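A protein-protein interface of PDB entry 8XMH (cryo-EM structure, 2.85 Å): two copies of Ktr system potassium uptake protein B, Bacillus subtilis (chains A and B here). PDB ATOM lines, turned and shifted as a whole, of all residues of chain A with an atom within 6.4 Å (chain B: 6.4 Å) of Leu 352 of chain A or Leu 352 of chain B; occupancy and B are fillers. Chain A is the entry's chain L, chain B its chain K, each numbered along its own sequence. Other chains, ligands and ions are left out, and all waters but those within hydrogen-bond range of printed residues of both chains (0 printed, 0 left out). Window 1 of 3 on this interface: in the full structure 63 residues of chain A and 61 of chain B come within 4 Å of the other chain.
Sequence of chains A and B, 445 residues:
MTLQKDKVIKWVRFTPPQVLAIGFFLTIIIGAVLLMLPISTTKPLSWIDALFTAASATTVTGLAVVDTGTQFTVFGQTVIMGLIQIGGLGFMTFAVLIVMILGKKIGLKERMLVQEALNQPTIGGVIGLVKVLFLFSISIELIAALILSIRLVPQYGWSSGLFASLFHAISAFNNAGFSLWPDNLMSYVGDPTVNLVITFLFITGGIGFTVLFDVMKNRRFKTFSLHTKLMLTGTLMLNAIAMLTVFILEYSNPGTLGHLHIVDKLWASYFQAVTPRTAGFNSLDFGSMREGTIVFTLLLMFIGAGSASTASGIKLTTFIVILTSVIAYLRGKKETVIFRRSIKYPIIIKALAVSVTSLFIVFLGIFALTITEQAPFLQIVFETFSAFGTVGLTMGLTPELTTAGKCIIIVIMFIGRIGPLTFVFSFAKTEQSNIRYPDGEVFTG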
ATOM      1  N   THR A 318      35.690 -20.881  26.936  1.00  0.00           N
ATOM      2  CA  THR A 318      34.318 -20.397  26.816  1.00  0.00           C
ATOM      3  C   THR A 318      34.289 -18.916  26.461  1.00  0.00           C
ATOM      4  O   THR A 318      33.484 -18.483  25.629  1.00  0.00           O
ATOM      5  CB  THR A 318      33.562 -20.651  28.120  1.00  0.00           C
ATOM      6  OG1 THR A 318      33.536 -22.056  28.389  1.00  0.00           O
ATOM      7  CG2 THR A 318      32.138 -20.136  28.037  1.00  0.00           C
ATOM      8  N   ILE A 322      32.889 -17.423  22.717  1.00  0.00           N
ATOM      9  CA  ILE A 322      31.818 -16.431  22.644  1.00  0.00           C
ATOM     10  C   ILE A 322      32.319 -15.142  22.008  1.00  0.00           C
ATOM     11  O   ILE A 322      31.632 -14.539  21.175  1.00  0.00           O
ATOM     12  CB  ILE A 322      31.236 -16.183  24.045  1.00  0.00           C
ATOM     13  CG1 ILE A 322      30.505 -17.425  24.537  1.00  0.00           C
ATOM     14  CG2 ILE A 322      30.297 -14.990  24.046  1.00  0.00           C
ATOM     15  CD1 ILE A 322      30.008 -17.296  25.937  1.00  0.00           C
ATOM     16  N   SER A 325      32.798 -15.648  18.308  1.00  0.00           N
ATOM     17  CA  SER A 325      31.524 -15.820  17.619  1.00  0.00           C
ATOM     18  C   SER A 325      30.840 -14.481  17.373  1.00  0.00           C
ATOM     19  O   SER A 325      30.195 -14.291  16.337  1.00  0.00           O
ATOM     20  CB  SER A 325      30.618 -16.748  18.426  1.00  0.00           C
ATOM     21  OG  SER A 325      29.350 -16.883  17.812  1.00  0.00           O
ATOM     22  N   VAL A 326      30.955 -13.548  18.320  1.00  0.00           N
ATOM     23  CA  VAL A 326      30.362 -12.226  18.146  1.00  0.00           C
ATOM     24  C   VAL A 326      31.117 -11.432  17.091  1.00  0.00           C
ATOM     25  O   VAL A 326      30.510 -10.799  16.222  1.00  0.00           O
ATOM     26  CB  VAL A 326      30.319 -11.485  19.493  1.00  0.00           C
ATOM     27  CG1 VAL A 326      29.829 -10.060  19.309  1.00  0.00           C
ATOM     28  CG2 VAL A 326      29.429 -12.223  20.463  1.00  0.00           C
ATOM     29  N   ILE A 347      29.065 -26.457  20.092  1.00  0.00           N
ATOM     30  CA  ILE A 347      30.077 -25.836  20.940  1.00  0.00           C
ATOM     31  C   ILE A 347      29.656 -24.424  21.330  1.00  0.00           C
ATOM     32  O   ILE A 347      29.890 -23.981  22.459  1.00  0.00           O
ATOM     33  CB  ILE A 347      31.443 -25.843  20.230  1.00  0.00           C
ATOM     34  CG1 ILE A 347      31.794 -27.251  19.749  1.00  0.00           C
ATOM     35  CG2 ILE A 347      32.528 -25.317  21.147  1.00  0.00           C
ATOM     36  CD1 ILE A 347      31.967 -28.250  20.857  1.00  0.00           C
ATOM     37  N   ILE A 348      29.033 -23.696  20.401  1.00  0.00           N
ATOM     38  CA  ILE A 348      28.627 -22.320  20.671  1.00  0.00           C
ATOM     39  C   ILE A 348      27.509 -22.278  21.702  1.00  0.00           C
ATOM     40  O   ILE A 348      27.533 -21.461  22.630  1.00  0.00           O
ATOM     41  CB  ILE A 348      28.211 -21.623  19.364  1.00  0.00           C
ATOM     42  CG1 ILE A 348      29.312 -21.734  18.312  1.00  0.00           C
ATOM     43  CG2 ILE A 348      27.874 -20.169  19.623  1.00  0.00           C
ATOM     44  CD1 ILE A 348      30.533 -20.936  18.624  1.00  0.00           C
ATOM     45  N   ILE A 349      26.508 -23.149  21.559  1.00  0.00           N
ATOM     46  CA  ILE A 349      25.349 -23.088  22.444  1.00  0.00           C
ATOM     47  C   ILE A 349      25.709 -23.555  23.851  1.00  0.00           C
ATOM     48  O   ILE A 349      25.109 -23.100  24.832  1.00  0.00           O
ATOM     49  CB  ILE A 349      24.174 -23.883  21.839  1.00  0.00           C
ATOM     50  CG1 ILE A 349      22.883 -23.612  22.614  1.00  0.00           C
ATOM     51  CG2 ILE A 349      24.475 -25.369  21.785  1.00  0.00           C
ATOM     52  CD1 ILE A 349      21.681 -24.348  22.074  1.00  0.00           C
ATOM     53  N   LYS A 350      26.688 -24.453  23.985  1.00  0.00           N
ATOM     54  CA  LYS A 350      27.138 -24.846  25.314  1.00  0.00           C
ATOM     55  C   LYS A 350      27.870 -23.705  26.008  1.00  0.00           C
ATOM     56  O   LYS A 350      27.700 -23.495  27.213  1.00  0.00           O
ATOM     57  CB  LYS A 350      28.029 -26.081  25.231  1.00  0.00           C
ATOM     58  CG  LYS A 350      28.438 -26.616  26.590  1.00  0.00           C
ATOM     59  CD  LYS A 350      29.253 -27.883  26.475  1.00  0.00           C
ATOM     60  CE  LYS A 350      29.655 -28.393  27.846  1.00  0.00           C
ATOM     61  NZ  LYS A 350      30.431 -29.659  27.762  1.00  0.00           N
ATOM     62  N   ALA A 351      28.692 -22.961  25.266  1.00  0.00           N
ATOM     63  CA  ALA A 351      29.344 -21.785  25.834  1.00  0.00           C
ATOM     64  C   ALA A 351      28.329 -20.703  26.170  1.00  0.00           C
ATOM     65  O   ALA A 351      28.492 -19.975  27.154  1.00  0.00           O
ATOM     66  CB  ALA A 351      30.397 -21.251  24.867  1.00  0.00           C
ATOM     67  N   LEU A 352      27.284 -20.577  25.352  1.00  0.00           N
ATOM     68  CA  LEU A 352      26.217 -19.624  25.633  1.00  0.00           C
ATOM     69  C   LEU A 352      25.485 -19.983  26.920  1.00  0.00           C
ATOM     70  O   LEU A 352      25.141 -19.101  27.714  1.00  0.00           O
ATOM     71  CB  LEU A 352      25.255 -19.575  24.443  1.00  0.00           C
ATOM     72  CG  LEU A 352      24.066 -18.609  24.347  1.00  0.00           C
ATOM     73  CD1 LEU A 352      22.774 -19.228  24.870  1.00  0.00           C
ATOM     74  CD2 LEU A 352      24.353 -17.294  25.047  1.00  0.00           C
ATOM     75  N   ALA A 353      25.236 -21.273  27.143  1.00  0.00           N
ATOM     76  CA  ALA A 353      24.522 -21.693  28.342  1.00  0.00           C
ATOM     77  C   ALA A 353      25.365 -21.519  29.598  1.00  0.00           C
ATOM     78  O   ALA A 353      24.822 -21.214  30.663  1.00  0.00           O
ATOM     79  CB  ALA A 353      24.072 -23.145  28.204  1.00  0.00           C
ATOM     80  N   VAL A 354      26.680 -21.718  29.500  1.00  0.00           N
ATOM     81  CA  VAL A 354      27.552 -21.556  30.659  1.00  0.00           C
ATOM     82  C   VAL A 354      27.609 -20.095  31.087  1.00  0.00           C
ATOM     83  O   VAL A 354      27.492 -19.774  32.274  1.00  0.00           O
ATOM     84  CB  VAL A 354      28.957 -22.104  30.351  1.00  0.00           C
ATOM     85  CG1 VAL A 354      29.943 -21.694  31.427  1.00  0.00           C
ATOM     86  CG2 VAL A 354      28.919 -23.609  30.226  1.00  0.00           C
ATOM     87  N   SER A 355      27.780 -19.189  30.124  1.00  0.00           N
ATOM     88  CA  SER A 355      27.971 -17.780  30.449  1.00  0.00           C
ATOM     89  C   SER A 355      26.690 -17.137  30.966  1.00  0.00           C
ATOM     90  O   SER A 355      26.734 -16.319  31.891  1.00  0.00           O
ATOM     91  CB  SER A 355      28.485 -17.035  29.223  1.00  0.00           C
ATOM     92  OG  SER A 355      28.649 -15.658  29.500  1.00  0.00           O
ATOM     93  N   VAL A 356      25.544 -17.476  30.376  1.00  0.00           N
ATOM     94  CA  VAL A 356      24.285 -16.877  30.806  1.00  0.00           C
ATOM     95  C   VAL A 356      23.882 -17.395  32.180  1.00  0.00           C
ATOM     96  O   VAL A 356      23.440 -16.626  33.041  1.00  0.00           O
ATOM     97  CB  VAL A 356      23.190 -17.127  29.753  1.00  0.00           C
ATOM     98  CG1 VAL A 356      21.830 -16.717  30.282  1.00  0.00           C
ATOM     99  CG2 VAL A 356      23.505 -16.358  28.489  1.00  0.00           C
ATOM    100  N   THR A 357      24.036 -18.699  32.415  1.00  0.00           N
ATOM    101  CA  THR A 357      23.684 -19.265  33.714  1.00  0.00           C
ATOM    102  C   THR A 357      24.599 -18.744  34.812  1.00  0.00           C
ATOM    103  O   THR A 357      24.153 -18.512  35.939  1.00  0.00           O
ATOM    104  CB  THR A 357      23.743 -20.789  33.660  1.00  0.00           C
ATOM    105  OG1 THR A 357      23.210 -21.243  32.411  1.00  0.00           O
ATOM    106  CG2 THR A 357      22.930 -21.391  34.788  1.00  0.00           C
ATOM    107  N   THR B 318      14.761  -9.657  22.904  1.00  0.00           N
ATOM    108  CA  THR B 318      16.119 -10.189  22.958  1.00  0.00           C
ATOM    109  C   THR B 318      16.359 -10.944  24.259  1.00  0.00           C
ATOM    110  O   THR B 318      16.979 -12.012  24.263  1.00  0.00           O
ATOM    111  CB  THR B 318      17.129  -9.054  22.801  1.00  0.00           C
ATOM    112  OG1 THR B 318      16.933  -8.413  21.537  1.00  0.00           O
ATOM    113  CG2 THR B 318      18.552  -9.572  22.878  1.00  0.00           C
ATOM    114  N   ILE B 322      16.971 -15.162  24.454  1.00  0.00           N
ATOM    115  CA  ILE B 322      18.164 -15.731  25.076  1.00  0.00           C
ATOM    116  C   ILE B 322      17.791 -16.585  26.280  1.00  0.00           C
ATOM    117  O   ILE B 322      18.337 -17.677  26.476  1.00  0.00           O
ATOM    118  CB  ILE B 322      19.144 -14.609  25.460  1.00  0.00           C
ATOM    119  CG1 ILE B 322      19.704 -13.953  24.205  1.00  0.00           C
ATOM    120  CG2 ILE B 322      20.274 -15.138  26.322  1.00  0.00           C
ATOM    121  CD1 ILE B 322      20.577 -12.780  24.499  1.00  0.00           C
ATOM    122  N   SER B 325      16.231 -19.811  25.123  1.00  0.00           N
ATOM    123  CA  SER B 325      17.207 -20.672  24.465  1.00  0.00           C
ATOM    124  C   SER B 325      18.063 -21.420  25.479  1.00  0.00           C
ATOM    125  O   SER B 325      18.428 -22.579  25.254  1.00  0.00           O
ATOM    126  CB  SER B 325      18.083 -19.846  23.526  1.00  0.00           C
ATOM    127  OG  SER B 325      19.080 -20.646  22.919  1.00  0.00           O
ATOM    128  N   VAL B 326      18.406 -20.771  26.592  1.00  0.00           N
ATOM    129  CA  VAL B 326      19.193 -21.427  27.631  1.00  0.00           C
ATOM    130  C   VAL B 326      18.362 -22.482  28.348  1.00  0.00           C
ATOM    131  O   VAL B 326      18.829 -23.601  28.586  1.00  0.00           O
ATOM    132  CB  VAL B 326      19.753 -20.382  28.612  1.00  0.00           C
ATOM    133  CG1 VAL B 326      20.460 -21.055  29.772  1.00  0.00           C
ATOM    134  CG2 VAL B 326      20.697 -19.451  27.892  1.00  0.00           C
ATOM    135  N   ILE B 347      17.966 -15.886  14.374  1.00  0.00           N
ATOM    136  CA  ILE B 347      17.374 -15.054  15.417  1.00  0.00           C
ATOM    137  C   ILE B 347      18.171 -15.172  16.711  1.00  0.00           C
ATOM    138  O   ILE B 347      18.350 -14.189  17.439  1.00  0.00           O
ATOM    139  CB  ILE B 347      15.898 -15.433  15.626  1.00  0.00           C
ATOM    140  CG1 ILE B 347      15.143 -15.417  14.297  1.00  0.00           C
ATOM    141  CG2 ILE B 347      15.237 -14.497  16.615  1.00  0.00           C
ATOM    142  CD1 ILE B 347      15.072 -14.062  13.651  1.00  0.00           C
ATOM    143  N   ILE B 348      18.657 -16.376  17.020  1.00  0.00           N
ATOM    144  CA  ILE B 348      19.398 -16.594  18.259  1.00  0.00           C
ATOM    145  C   ILE B 348      20.738 -15.871  18.221  1.00  0.00           C
ATOM    146  O   ILE B 348      21.137 -15.227  19.197  1.00  0.00           O
ATOM    147  CB  ILE B 348      19.582 -18.101  18.511  1.00  0.00           C
ATOM    148  CG1 ILE B 348      18.238 -18.827  18.474  1.00  0.00           C
ATOM    149  CG2 ILE B 348      20.272 -18.335  19.839  1.00  0.00           C
ATOM    150  CD1 ILE B 348      17.342 -18.503  19.624  1.00  0.00           C
ATOM    151  N   ILE B 349      21.458 -15.969  17.102  1.00  0.00           N
ATOM    152  CA  ILE B 349      22.799 -15.399  17.039  1.00  0.00           C
ATOM    153  C   ILE B 349      22.745 -13.874  17.008  1.00  0.00           C
ATOM    154  O   ILE B 349      23.669 -13.207  17.488  1.00  0.00           O
ATOM    155  CB  ILE B 349      23.573 -15.987  15.841  1.00  0.00           C
ATOM    156  CG1 ILE B 349      25.052 -15.605  15.914  1.00  0.00           C
ATOM    157  CG2 ILE B 349      22.965 -15.559  14.518  1.00  0.00           C
ATOM    158  CD1 ILE B 349      25.883 -16.155  14.780  1.00  0.00           C
ATOM    159  N   LYS B 350      21.674 -13.293  16.462  1.00  0.00           N
ATOM    160  CA  LYS B 350      21.529 -11.843  16.508  1.00  0.00           C
ATOM    161  C   LYS B 350      21.267 -11.361  17.928  1.00  0.00           C
ATOM    162  O   LYS B 350      21.797 -10.326  18.344  1.00  0.00           O
ATOM    163  CB  LYS B 350      20.411 -11.390  15.574  1.00  0.00           C
ATOM    164  CG  LYS B 350      20.283  -9.881  15.484  1.00  0.00           C
ATOM    165  CD  LYS B 350      19.221  -9.465  14.493  1.00  0.00           C
ATOM    166  CE  LYS B 350      19.110  -7.954  14.425  1.00  0.00           C
ATOM    167  NZ  LYS B 350      18.093  -7.517  13.431  1.00  0.00           N
ATOM    168  N   ALA B 351      20.450 -12.095  18.686  1.00  0.00           N
ATOM    169  CA  ALA B 351      20.236 -11.755  20.089  1.00  0.00           C
ATOM    170  C   ALA B 351      21.506 -11.955  20.901  1.00  0.00           C
ATOM    171  O   ALA B 351      21.773 -11.204  21.845  1.00  0.00           O
ATOM    172  CB  ALA B 351      19.096 -12.593  20.664  1.00  0.00           C
ATOM    173  N   LEU B 352      22.293 -12.975  20.556  1.00  0.00           N
ATOM    174  CA  LEU B 352      23.571 -13.200  21.221  1.00  0.00           C
ATOM    175  C   LEU B 352      24.533 -12.046  20.969  1.00  0.00           C
ATOM    176  O   LEU B 352      25.256 -11.621  21.876  1.00  0.00           O
ATOM    177  CB  LEU B 352      24.163 -14.530  20.744  1.00  0.00           C
ATOM    178  CG  LEU B 352      25.456 -15.137  21.304  1.00  0.00           C
ATOM    179  CD1 LEU B 352      26.683 -14.742  20.488  1.00  0.00           C
ATOM    180  CD2 LEU B 352      25.650 -14.790  22.768  1.00  0.00           C
ATOM    181  N   ALA B 353      24.557 -11.527  19.740  1.00  0.00           N
ATOM    182  CA  ALA B 353      25.466 -10.434  19.418  1.00  0.00           C
ATOM    183  C   ALA B 353      25.051  -9.131  20.085  1.00  0.00           C
ATOM    184  O   ALA B 353      25.913  -8.332  20.458  1.00  0.00           O
ATOM    185  CB  ALA B 353      25.549 -10.250  17.904  1.00  0.00           C
ATOM    186  N   VAL B 354      23.747  -8.894  20.235  1.00  0.00           N
ATOM    187  CA  VAL B 354      23.276  -7.671  20.879  1.00  0.00           C
ATOM    188  C   VAL B 354      23.644  -7.668  22.357  1.00  0.00           C
ATOM    189  O   VAL B 354      24.141  -6.669  22.887  1.00  0.00           O
ATOM    190  CB  VAL B 354      21.758  -7.514  20.679  1.00  0.00           C
ATOM    191  CG1 VAL B 354      21.208  -6.415  21.568  1.00  0.00           C
ATOM    192  CG2 VAL B 354      21.445  -7.218  19.232  1.00  0.00           C
ATOM    193  N   SER B 355      23.411  -8.789  23.040  1.00  0.00           N
ATOM    194  CA  SER B 355      23.613  -8.839  24.484  1.00  0.00           C
ATOM    195  C   SER B 355      25.091  -8.801  24.853  1.00  0.00           C
ATOM    196  O   SER B 355      25.471  -8.155  25.835  1.00  0.00           O
ATOM    197  CB  SER B 355      22.953 -10.090  25.052  1.00  0.00           C
ATOM    198  OG  SER B 355      23.162 -10.183  26.448  1.00  0.00           O
ATOM    199  N   VAL B 356      25.938  -9.498  24.093  1.00  0.00           N
ATOM    200  CA  VAL B 356      27.362  -9.524  24.407  1.00  0.00           C
ATOM    201  C   VAL B 356      28.005  -8.174  24.115  1.00  0.00           C
ATOM    202  O   VAL B 356      28.814  -7.676  24.905  1.00  0.00           O
ATOM    203  CB  VAL B 356      28.054 -10.669  23.645  1.00  0.00           C
ATOM    204  CG1 VAL B 356      29.561 -10.571  23.775  1.00  0.00           C
ATOM    205  CG2 VAL B 356      27.575 -12.004  24.173  1.00  0.00           C
ATOM    206  N   THR B 357      27.651  -7.558  22.986  1.00  0.00           N
ATOM    207  CA  THR B 357      28.216  -6.255  22.646  1.00  0.00           C
ATOM    208  C   THR B 357      27.762  -5.182  23.625  1.00  0.00           C
ATOM    209  O   THR B 357      28.536  -4.283  23.969  1.00  0.00           O
ATOM    210  CB  THR B 357      27.828  -5.866  21.222  1.00  0.00           C
ATOM    211  OG1 THR B 357      27.896  -7.020  20.378  1.00  0.00           O
ATOM    212  CG2 THR B 357      28.773  -4.809  20.685  1.00  0.00           C
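Among the printed residues, merely in contact across the chains: Val 326 of chain A with Leu 352 of chain B, Val 326 of chain A with Val 356 of chain B, Val 326 of chain A with Thr 357 of chain B, Leu 352 of chain A with Val 326 of chain B, Leu 352 of chain A with Leu 352 of chain B, Val 356 of chain A with Val 326 of chain B and Thr 357 of chain A with Val 326 of chain B.
Printed residues of chain B within 4 Å of Leu 352 of chain A: Val 326 and Leu 352. Of chain A, only Val 326 (3.7 Å) and Leu 352 (3.6 Å) come within 4 Å of Leu 352 of chain B. Printed residues of chain B within 4 Å of Val 356 of chain A: Val 326. Printed residues of chain B within 4 Å of Thr 357 of chain A: Val 326 (3.8 Å). Of the printed residues of chain B, Val 326 of chain A touches Leu 352 (3.7 Å), Val 356 (3.7 Å) and Thr 357 (3.8 Å). Printed residues of chain A within 4 Å of Thr 357 of chain B: Val 326 (3.8 Å). Ala 353 of chain A touches none of the printed residues of chain B. The nearest residue of chain B that does not touch Leu 352 of chain A is Ser 325 of chain B (4.4 Å).
Hydrophobic or aromatic side chains of chain B that line the printed part of chain A: Val 326, Leu 352 and Val 356. Along chain B the printed residues that touch a printed residue of chain A span positions 326 to 357. Hydrophobic or aromatic side chains of chain A within 4 Å of the printed part of chain B: Val 326, Leu 352 and Val 356. Among the printed residues, 7 pairs touch across the chains.
Val 326 of chain A touches Leu 352 of chain B, and with the chains exchanged Leu 352 of chain A touches Val 326 of chain B. Val 326 of chain A touches Val 356 of chain B, and with the chains exchanged Val 356 of chain A touches Val 326 of chain B. Val 326 of chain A touches Thr 357 of chain B, and with the chains exchanged Thr 357 of chain A touches Val 326 of chain B. Leu 352 of chain A touches its own counterpart, Leu 352 of chain B. Of the 7 pairs that touch across the chains among the printed residues, 7 have their exchanged pair printed and touching as well.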
